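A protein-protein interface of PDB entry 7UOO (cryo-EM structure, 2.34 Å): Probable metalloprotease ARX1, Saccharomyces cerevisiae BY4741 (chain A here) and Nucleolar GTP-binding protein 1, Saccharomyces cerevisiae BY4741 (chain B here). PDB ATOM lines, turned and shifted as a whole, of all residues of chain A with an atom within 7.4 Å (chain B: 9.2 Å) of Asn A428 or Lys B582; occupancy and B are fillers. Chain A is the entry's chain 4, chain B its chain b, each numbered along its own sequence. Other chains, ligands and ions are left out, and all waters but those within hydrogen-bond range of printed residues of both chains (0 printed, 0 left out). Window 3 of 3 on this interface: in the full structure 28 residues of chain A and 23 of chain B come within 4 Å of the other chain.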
ATOM      1  N   HIS A 368       5.787  -9.694 -18.778  1.00  0.00           N
ATOM      2  CA  HIS A 368       5.717  -8.250 -18.952  1.00  0.00           C
ATOM      3  C   HIS A 368       6.762  -7.612 -18.051  1.00  0.00           C
ATOM      4  O   HIS A 368       6.772  -7.863 -16.844  1.00  0.00           O
ATOM      5  CB  HIS A 368       4.318  -7.717 -18.618  1.00  0.00           C
ATOM      6  CG  HIS A 368       4.205  -6.227 -18.694  1.00  0.00           C
ATOM      7  ND1 HIS A 368       4.469  -5.406 -17.618  1.00  0.00           N
ATOM      8  CD2 HIS A 368       3.859  -5.410 -19.715  1.00  0.00           C
ATOM      9  CE1 HIS A 368       4.290  -4.147 -17.975  1.00  0.00           C
ATOM     10  NE2 HIS A 368       3.918  -4.122 -19.242  1.00  0.00           N
ATOM     11  N   LEU A 370       8.450  -5.082 -15.751  1.00  0.00           N
ATOM     12  CA  LEU A 370       7.890  -4.110 -14.827  1.00  0.00           C
ATOM     13  C   LEU A 370       8.748  -2.854 -14.763  1.00  0.00           C
ATOM     14  O   LEU A 370       9.965  -2.891 -14.963  1.00  0.00           O
ATOM     15  CB  LEU A 370       7.754  -4.706 -13.424  1.00  0.00           C
ATOM     16  CG  LEU A 370       6.818  -5.898 -13.194  1.00  0.00           C
ATOM     17  CD1 LEU A 370       5.571  -5.813 -14.060  1.00  0.00           C
ATOM     18  CD2 LEU A 370       7.540  -7.211 -13.397  1.00  0.00           C
ATOM     19  N   LYS A 371       8.092  -1.730 -14.476  1.00  0.00           N
ATOM     20  CA  LYS A 371       8.798  -0.461 -14.360  1.00  0.00           C
ATOM     21  C   LYS A 371       9.550  -0.333 -13.038  1.00  0.00           C
ATOM     22  O   LYS A 371      10.620   0.283 -13.001  1.00  0.00           O
ATOM     23  CB  LYS A 371       7.815   0.703 -14.514  1.00  0.00           C
ATOM     24  CG  LYS A 371       6.968   0.660 -15.780  1.00  0.00           C
ATOM     25  CD  LYS A 371       7.816   0.766 -17.042  1.00  0.00           C
ATOM     26  CE  LYS A 371       6.944   0.945 -18.279  1.00  0.00           C
ATOM     27  NZ  LYS A 371       7.743   1.075 -19.531  1.00  0.00           N
ATOM     28  N   GLY A 422       5.559  -3.759  -4.543  1.00  0.00           N
ATOM     29  CA  GLY A 422       5.877  -4.495  -5.762  1.00  0.00           C
ATOM     30  C   GLY A 422       4.709  -5.311  -6.292  1.00  0.00           C
ATOM     31  O   GLY A 422       4.491  -5.395  -7.509  1.00  0.00           O
ATOM     32  N   MET A 423       3.945  -5.924  -5.387  1.00  0.00           N
ATOM     33  CA  MET A 423       2.827  -6.772  -5.777  1.00  0.00           C
ATOM     34  C   MET A 423       1.730  -5.974  -6.462  1.00  0.00           C
ATOM     35  O   MET A 423       1.000  -6.519  -7.295  1.00  0.00           O
ATOM     36  CB  MET A 423       2.278  -7.493  -4.546  1.00  0.00           C
ATOM     37  CG  MET A 423       1.267  -8.581  -4.845  1.00  0.00           C
ATOM     38  SD  MET A 423       1.967  -9.939  -5.799  1.00  0.00           S
ATOM     39  CE  MET A 423       0.778 -10.025  -7.126  1.00  0.00           C
ATOM     40  N   SER A 424       1.597  -4.688  -6.125  1.00  0.00           N
ATOM     41  CA  SER A 424       0.596  -3.860  -6.791  1.00  0.00           C
ATOM     42  C   SER A 424       0.853  -3.779  -8.293  1.00  0.00           C
ATOM     43  O   SER A 424      -0.074  -3.918  -9.099  1.00  0.00           O
ATOM     44  CB  SER A 424       0.576  -2.464  -6.179  1.00  0.00           C
ATOM     45  OG  SER A 424       1.788  -1.778  -6.434  1.00  0.00           O
ATOM     46  N   GLU A 425       2.109  -3.561  -8.692  1.00  0.00           N
ATOM     47  CA  GLU A 425       2.405  -3.526 -10.119  1.00  0.00           C
ATOM     48  C   GLU A 425       2.455  -4.920 -10.729  1.00  0.00           C
ATOM     49  O   GLU A 425       2.169  -5.072 -11.922  1.00  0.00           O
ATOM     50  CB  GLU A 425       3.725  -2.803 -10.394  1.00  0.00           C
ATOM     51  CG  GLU A 425       3.844  -2.349 -11.847  1.00  0.00           C
ATOM     52  CD  GLU A 425       5.256  -1.997 -12.260  1.00  0.00           C
ATOM     53  OE1 GLU A 425       6.208  -2.391 -11.558  1.00  0.00           O
ATOM     54  OE2 GLU A 425       5.416  -1.327 -13.300  1.00  0.00           O
ATOM     55  N   ILE A 426       2.824  -5.939  -9.948  1.00  0.00           N
ATOM     56  CA  ILE A 426       2.838  -7.300 -10.485  1.00  0.00           C
ATOM     57  C   ILE A 426       1.426  -7.747 -10.853  1.00  0.00           C
ATOM     58  O   ILE A 426       1.187  -8.270 -11.948  1.00  0.00           O
ATOM     59  CB  ILE A 426       3.499  -8.271  -9.488  1.00  0.00           C
ATOM     60  CG1 ILE A 426       5.007  -8.030  -9.430  1.00  0.00           C
ATOM     61  CG2 ILE A 426       3.217  -9.711  -9.881  1.00  0.00           C
ATOM     62  CD1 ILE A 426       5.752  -8.957  -8.499  1.00  0.00           C
ATOM     63  N   SER A 427       0.462  -7.525  -9.956  1.00  0.00           N
ATOM     64  CA  SER A 427      -0.901  -7.987 -10.205  1.00  0.00           C
ATOM     65  C   SER A 427      -1.602  -7.154 -11.272  1.00  0.00           C
ATOM     66  O   SER A 427      -2.455  -7.678 -11.997  1.00  0.00           O
ATOM     67  CB  SER A 427      -1.710  -7.968  -8.908  1.00  0.00           C
ATOM     68  OG  SER A 427      -1.774  -6.661  -8.371  1.00  0.00           O
ATOM     69  N   ASN A 428      -1.262  -5.867 -11.383  1.00  0.00           N
ATOM     70  CA  ASN A 428      -1.906  -4.987 -12.352  1.00  0.00           C
ATOM     71  C   ASN A 428      -1.591  -5.373 -13.793  1.00  0.00           C
ATOM     72  O   ASN A 428      -2.383  -5.070 -14.690  1.00  0.00           O
ATOM     73  CB  ASN A 428      -1.486  -3.538 -12.097  1.00  0.00           C
ATOM     74  CG  ASN A 428      -2.426  -2.533 -12.737  1.00  0.00           C
ATOM     75  OD1 ASN A 428      -3.636  -2.739 -12.788  1.00  0.00           O
ATOM     76  ND2 ASN A 428      -1.869  -1.436 -13.229  1.00  0.00           N
ATOM     77  N   ASN A 429      -0.464  -6.040 -14.033  1.00  0.00           N
ATOM     78  CA  ASN A 429      -0.089  -6.502 -15.361  1.00  0.00           C
ATOM     79  C   ASN A 429      -0.369  -7.987 -15.559  1.00  0.00           C
ATOM     80  O   ASN A 429       0.186  -8.596 -16.480  1.00  0.00           O
ATOM     81  CB  ASN A 429       1.383  -6.193 -15.627  1.00  0.00           C
ATOM     82  CG  ASN A 429       1.678  -4.710 -15.572  1.00  0.00           C
ATOM     83  OD1 ASN A 429       1.308  -3.962 -16.473  1.00  0.00           O
ATOM     84  ND2 ASN A 429       2.342  -4.278 -14.509  1.00  0.00           N
ATOM     85  N   TYR A 430      -1.200  -8.577 -14.698  1.00  0.00           N
ATOM     86  CA  TYR A 430      -1.696  -9.950 -14.814  1.00  0.00           C
ATOM     87  C   TYR A 430      -0.589 -10.999 -14.731  1.00  0.00           C
ATOM     88  O   TYR A 430      -0.751 -12.109 -15.244  1.00  0.00           O
ATOM     89  CB  TYR A 430      -2.502 -10.149 -16.105  1.00  0.00           C
ATOM     90  CG  TYR A 430      -3.578  -9.115 -16.324  1.00  0.00           C
ATOM     91  CD1 TYR A 430      -4.727  -9.109 -15.549  1.00  0.00           C
ATOM     92  CD2 TYR A 430      -3.447  -8.148 -17.311  1.00  0.00           C
ATOM     93  CE1 TYR A 430      -5.716  -8.170 -15.748  1.00  0.00           C
ATOM     94  CE2 TYR A 430      -4.431  -7.204 -17.518  1.00  0.00           C
ATOM     95  CZ  TYR A 430      -5.563  -7.220 -16.735  1.00  0.00           C
ATOM     96  OH  TYR A 430      -6.546  -6.284 -16.937  1.00  0.00           O
ATOM     97  N   LEU A 431       0.539 -10.682 -14.094  1.00  0.00           N
ATOM     98  CA  LEU A 431       1.579 -11.688 -13.911  1.00  0.00           C
ATOM     99  C   LEU A 431       1.234 -12.665 -12.794  1.00  0.00           C
ATOM    100  O   LEU A 431       1.607 -13.840 -12.869  1.00  0.00           O
ATOM    101  CB  LEU A 431       2.926 -11.020 -13.635  1.00  0.00           C
ATOM    102  CG  LEU A 431       3.468 -10.103 -14.735  1.00  0.00           C
ATOM    103  CD1 LEU A 431       4.886  -9.654 -14.423  1.00  0.00           C
ATOM    104  CD2 LEU A 431       3.407 -10.777 -16.094  1.00  0.00           C
ATOM    105  N   CYS A 432       0.532 -12.202 -11.762  1.00  0.00           N
ATOM    106  CA  CYS A 432       0.080 -13.047 -10.667  1.00  0.00           C
ATOM    107  C   CYS A 432      -1.384 -12.764 -10.370  1.00  0.00           C
ATOM    108  O   CYS A 432      -1.857 -11.635 -10.520  1.00  0.00           O
ATOM    109  CB  CYS A 432       0.906 -12.830  -9.396  1.00  0.00           C
ATOM    110  SG  CYS A 432       2.607 -13.406  -9.481  1.00  0.00           S
ATOM    111  N   THR B 574      -5.963 -15.446 -17.947  1.00  0.00           N
ATOM    112  CA  THR B 574      -6.589 -14.164 -17.673  1.00  0.00           C
ATOM    113  C   THR B 574      -7.523 -13.829 -18.824  1.00  0.00           C
ATOM    114  O   THR B 574      -7.167 -14.010 -19.992  1.00  0.00           O
ATOM    115  CB  THR B 574      -5.532 -13.060 -17.491  1.00  0.00           C
ATOM    116  OG1 THR B 574      -4.879 -13.226 -16.226  1.00  0.00           O
ATOM    117  CG2 THR B 574      -6.156 -11.677 -17.555  1.00  0.00           C
ATOM    118  N   ALA B 575      -8.730 -13.373 -18.487  1.00  0.00           N
ATOM    119  CA  ALA B 575      -9.668 -12.897 -19.495  1.00  0.00           C
ATOM    120  C   ALA B 575      -9.091 -11.690 -20.220  1.00  0.00           C
ATOM    121  O   ALA B 575      -8.944 -10.617 -19.626  1.00  0.00           O
ATOM    122  CB  ALA B 575     -11.010 -12.543 -18.854  1.00  0.00           C
ATOM    123  N   THR B 577      -8.938  -8.469 -22.102  1.00  0.00           N
ATOM    124  CA  THR B 577      -9.894  -7.377 -22.203  1.00  0.00           C
ATOM    125  C   THR B 577     -10.088  -6.953 -23.653  1.00  0.00           C
ATOM    126  O   THR B 577      -9.216  -7.143 -24.506  1.00  0.00           O
ATOM    127  CB  THR B 577      -9.427  -6.184 -21.371  1.00  0.00           C
ATOM    128  OG1 THR B 577      -8.127  -5.775 -21.813  1.00  0.00           O
ATOM    129  CG2 THR B 577      -9.358  -6.556 -19.899  1.00  0.00           C
ATOM    130  N   GLU B 578     -11.259  -6.376 -23.930  1.00  0.00           N
ATOM    131  CA  GLU B 578     -11.575  -5.938 -25.283  1.00  0.00           C
ATOM    132  C   GLU B 578     -10.809  -4.686 -25.689  1.00  0.00           C
ATOM    133  O   GLU B 578     -10.633  -4.448 -26.888  1.00  0.00           O
ATOM    134  CB  GLU B 578     -13.080  -5.687 -25.423  1.00  0.00           C
ATOM    135  CG  GLU B 578     -13.942  -6.938 -25.346  1.00  0.00           C
ATOM    136  CD  GLU B 578     -14.335  -7.301 -23.926  1.00  0.00           C
ATOM    137  OE1 GLU B 578     -14.520  -6.379 -23.103  1.00  0.00           O
ATOM    138  OE2 GLU B 578     -14.458  -8.509 -23.632  1.00  0.00           O
ATOM    139  N   ASN B 579     -10.352  -3.883 -24.728  1.00  0.00           N
ATOM    140  CA  ASN B 579      -9.683  -2.622 -25.017  1.00  0.00           C
ATOM    141  C   ASN B 579      -8.212  -2.622 -24.623  1.00  0.00           C
ATOM    142  O   ASN B 579      -7.578  -1.564 -24.650  1.00  0.00           O
ATOM    143  CB  ASN B 579     -10.405  -1.468 -24.319  1.00  0.00           C
ATOM    144  CG  ASN B 579     -11.476  -0.843 -25.186  1.00  0.00           C
ATOM    145  OD1 ASN B 579     -11.246  -0.550 -26.357  1.00  0.00           O
ATOM    146  ND2 ASN B 579     -12.654  -0.636 -24.616  1.00  0.00           N
ATOM    147  N   GLY B 580      -7.657  -3.775 -24.263  1.00  0.00           N
ATOM    148  CA  GLY B 580      -6.256  -3.847 -23.872  1.00  0.00           C
ATOM    149  C   GLY B 580      -5.920  -3.047 -22.631  1.00  0.00           C
ATOM    150  O   GLY B 580      -4.870  -2.398 -22.580  1.00  0.00           O
ATOM    151  N   VAL B 581      -6.788  -3.083 -21.629  1.00  0.00           N
ATOM    152  CA  VAL B 581      -6.613  -2.273 -20.434  1.00  0.00           C
ATOM    153  C   VAL B 581      -5.905  -3.087 -19.358  1.00  0.00           C
ATOM    154  O   VAL B 581      -5.889  -4.320 -19.381  1.00  0.00           O
ATOM    155  CB  VAL B 581      -7.965  -1.734 -19.923  1.00  0.00           C
ATOM    156  CG1 VAL B 581      -8.667  -0.955 -21.020  1.00  0.00           C
ATOM    157  CG2 VAL B 581      -8.845  -2.873 -19.427  1.00  0.00           C
ATOM    158  N   LYS B 582      -5.304  -2.383 -18.402  1.00  0.00           N
ATOM    159  CA  LYS B 582      -4.693  -3.013 -17.242  1.00  0.00           C
ATOM    160  C   LYS B 582      -5.770  -3.395 -16.228  1.00  0.00           C
ATOM    161  O   LYS B 582      -6.958  -3.111 -16.408  1.00  0.00           O
ATOM    162  CB  LYS B 582      -3.652  -2.087 -16.616  1.00  0.00           C
ATOM    163  CG  LYS B 582      -2.376  -1.930 -17.428  1.00  0.00           C
ATOM    164  CD  LYS B 582      -1.362  -1.069 -16.692  1.00  0.00           C
ATOM    165  CE  LYS B 582      -0.004  -1.078 -17.380  1.00  0.00           C
ATOM    166  NZ  LYS B 582      -0.013  -0.360 -18.685  1.00  0.00           N
ATOM    167  N   LEU B 583      -5.347  -4.052 -15.145  1.00  0.00           N
ATOM    168  CA  LEU B 583      -6.295  -4.576 -14.164  1.00  0.00           C
ATOM    169  C   LEU B 583      -7.087  -3.464 -13.487  1.00  0.00           C
ATOM    170  O   LEU B 583      -8.306  -3.577 -13.316  1.00  0.00           O
ATOM    171  CB  LEU B 583      -5.558  -5.416 -13.120  1.00  0.00           C
ATOM    172  CG  LEU B 583      -6.389  -5.939 -11.945  1.00  0.00           C
ATOM    173  CD1 LEU B 583      -7.447  -6.921 -12.424  1.00  0.00           C
ATOM    174  CD2 LEU B 583      -5.498  -6.576 -10.891  1.00  0.00           C
ATOM    175  N   ARG B 584      -6.419  -2.379 -13.102  1.00  0.00           N
ATOM    176  CA  ARG B 584      -7.062  -1.274 -12.404  1.00  0.00           C
ATOM    177  C   ARG B 584      -7.191  -0.037 -13.288  1.00  0.00           C
ATOM    178  O   ARG B 584      -7.071   1.093 -12.813  1.00  0.00           O
ATOM    179  CB  ARG B 584      -6.301  -0.949 -11.119  1.00  0.00           C
ATOM    180  CG  ARG B 584      -6.224  -2.129 -10.168  1.00  0.00           C
ATOM    181  CD  ARG B 584      -5.381  -1.828  -8.948  1.00  0.00           C
ATOM    182  NE  ARG B 584      -5.219  -3.010  -8.111  1.00  0.00           N
ATOM    183  CZ  ARG B 584      -4.144  -3.786  -8.110  1.00  0.00           C
ATOM    184  NH1 ARG B 584      -3.101  -3.523  -8.879  1.00  0.00           N
ATOM    185  NH2 ARG B 584      -4.115  -4.854  -7.318  1.00  0.00           N
ATOM    186  N   GLN B 585      -7.433  -0.244 -14.578  1.00  0.00           N
ATOM    187  CA  GLN B 585      -7.624   0.834 -15.536  1.00  0.00           C
ATOM    188  C   GLN B 585      -9.109   0.975 -15.839  1.00  0.00           C
ATOM    189  O   GLN B 585      -9.797  -0.025 -16.058  1.00  0.00           O
ATOM    190  CB  GLN B 585      -6.835   0.559 -16.819  1.00  0.00           C
ATOM    191  CG  GLN B 585      -7.039   1.574 -17.926  1.00  0.00           C
ATOM    192  CD  GLN B 585      -6.207   1.264 -19.155  1.00  0.00           C
ATOM    193  OE1 GLN B 585      -5.277   0.461 -19.100  1.00  0.00           O
ATOM    194  NE2 GLN B 585      -6.540   1.894 -20.270  1.00  0.00           N
ATOM    195  N   THR B 586      -9.600   2.211 -15.840  1.00  0.00           N
ATOM    196  CA  THR B 586     -10.998   2.450 -16.163  1.00  0.00           C
ATOM    197  C   THR B 586     -11.259   2.199 -17.644  1.00  0.00           C
ATOM    198  O   THR B 586     -10.407   2.446 -18.502  1.00  0.00           O
ATOM    199  CB  THR B 586     -11.404   3.881 -15.806  1.00  0.00           C
ATOM    200  OG1 THR B 586     -10.704   4.804 -16.649  1.00  0.00           O
ATOM    201  CG2 THR B 586     -11.079   4.187 -14.353  1.00  0.00           C
ATOM    202  N   ASP B 587     -12.449   1.687 -17.939  1.00  0.00           N
ATOM    203  CA  ASP B 587     -12.928   1.532 -19.311  1.00  0.00           C
ATOM    204  C   ASP B 587     -14.183   2.388 -19.432  1.00  0.00           C
ATOM    205  O   ASP B 587     -15.261   1.992 -18.982  1.00  0.00           O
ATOM    206  CB  ASP B 587     -13.194   0.068 -19.656  1.00  0.00           C
ATOM    207  CG  ASP B 587     -13.271  -0.179 -21.157  1.00  0.00           C
ATOM    208  OD1 ASP B 587     -13.789   0.689 -21.892  1.00  0.00           O
ATOM    209  OD2 ASP B 587     -12.807  -1.248 -21.606  1.00  0.00           O
ATOM    210  N   ASP B 591     -17.614  -0.172 -18.771  1.00  0.00           N
ATOM    211  CA  ASP B 591     -17.744  -0.422 -17.338  1.00  0.00           C
ATOM    212  C   ASP B 591     -19.196  -0.499 -16.878  1.00  0.00           C
ATOM    213  O   ASP B 591     -19.468  -1.118 -15.845  1.00  0.00           O
ATOM    214  CB  ASP B 591     -17.005   0.652 -16.538  1.00  0.00           C
ATOM    215  CG  ASP B 591     -15.523   0.356 -16.394  1.00  0.00           C
ATOM    216  OD1 ASP B 591     -15.077  -0.707 -16.873  1.00  0.00           O
ATOM    217  OD2 ASP B 591     -14.803   1.188 -15.805  1.00  0.00           O
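O of Val B581 sits at hydrogen-bond distance from OH of Tyr A430, at 3.2 Å.
OH of Tyr A430 lies close to O of Lys B582.
N of Leu B583 sits at hydrogen-bond distance from O of Asn A428 (3.2 Å).
N of Leu B583 lies within hydrogen-bond range of OH of Tyr A430, 3.1 Å away.
The guanidinium group (NH1) of Arg B584 is in hydrogen-bond range of the backbone carbonyl oxygen (O) of Ser A424 (3.1 Å).
The guanidinium group (NH2) of Arg B584 sits at hydrogen-bond distance from the side-chain hydroxyl (OG) of Ser A427.
The side-chain amide oxygen of Asn A428 is in hydrogen-bond range of the backbone NH of Arg B584.
Among the printed residues, merely in contact across the chains: Ser A427 with Leu B583 (3.4 Å), Asn A428 with Lys B582 (3.5 Å), Asn A429 with Lys B582 (3.3 Å) and Tyr A430 with Thr B574 (3.6 Å).
Of the 14 printed residues of chain A, 5 touch a printed residue of chain B.
Printed residues of chain A that touch a printed residue of chain B: Ser A424, Ser A427, Asn A428, Asn A429 and Tyr A430.
Among the printed residues, 11 pairs touch across the chains.
N of Val B581 sits at hydrogen-bond distance from OG1 of Thr B577 (3.0 Å).
N of Lys B582 lies within hydrogen-bond range of OE1 of Gln B585.
The backbone carbonyl oxygen (O) of Met A423 lies within hydrogen-bond range of the side-chain hydroxyl (OG) of Ser A427 (3.0 Å).
The side-chain hydroxyl (OG) of Ser A427 is in hydrogen-bond range of the backbone carbonyl oxygen (O) of Ser A424 (3.3 Å).
The backbone carbonyl oxygen of Glu A425 sits at hydrogen-bond distance from the side-chain amide nitrogen of Asn A429.
Leu A370 touches none of the printed residues of chain B.
Printed residues of chain B within 4 Å of Ser A424: Arg B584 (3.1 Å).
Of chain B, only Lys B582, Leu B583 and Arg B584 come within 4 Å of Asn A428.
Asn A429 touches one residue of chain B.
Of the printed residues of chain B, Tyr A430 touches Thr B574, Val B581, Lys B582 and Leu B583.
Of the printed residues of chain A, Val B581 touches Tyr A430 (3.2 Å).
Of chain A, only Asn A428 (3.5 Å), Asn A429 (3.3 Å) and Tyr A430 (3.1 Å) come within 4 Å of Lys B582.
Printed residues of chain A within 4 Å of Leu B583: Ser A427, Asn A428 and Tyr A430.
Of the printed residues of chain A, Arg B584 touches Ser A424, Ser A427 and Asn A428.
The nearest residue of chain B that does not touch Asn A428 is Gln B585 (4.9 Å).
The nearest printed residue of chain A that does not touch Val B581 is Asn A428 (5.9 Å).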
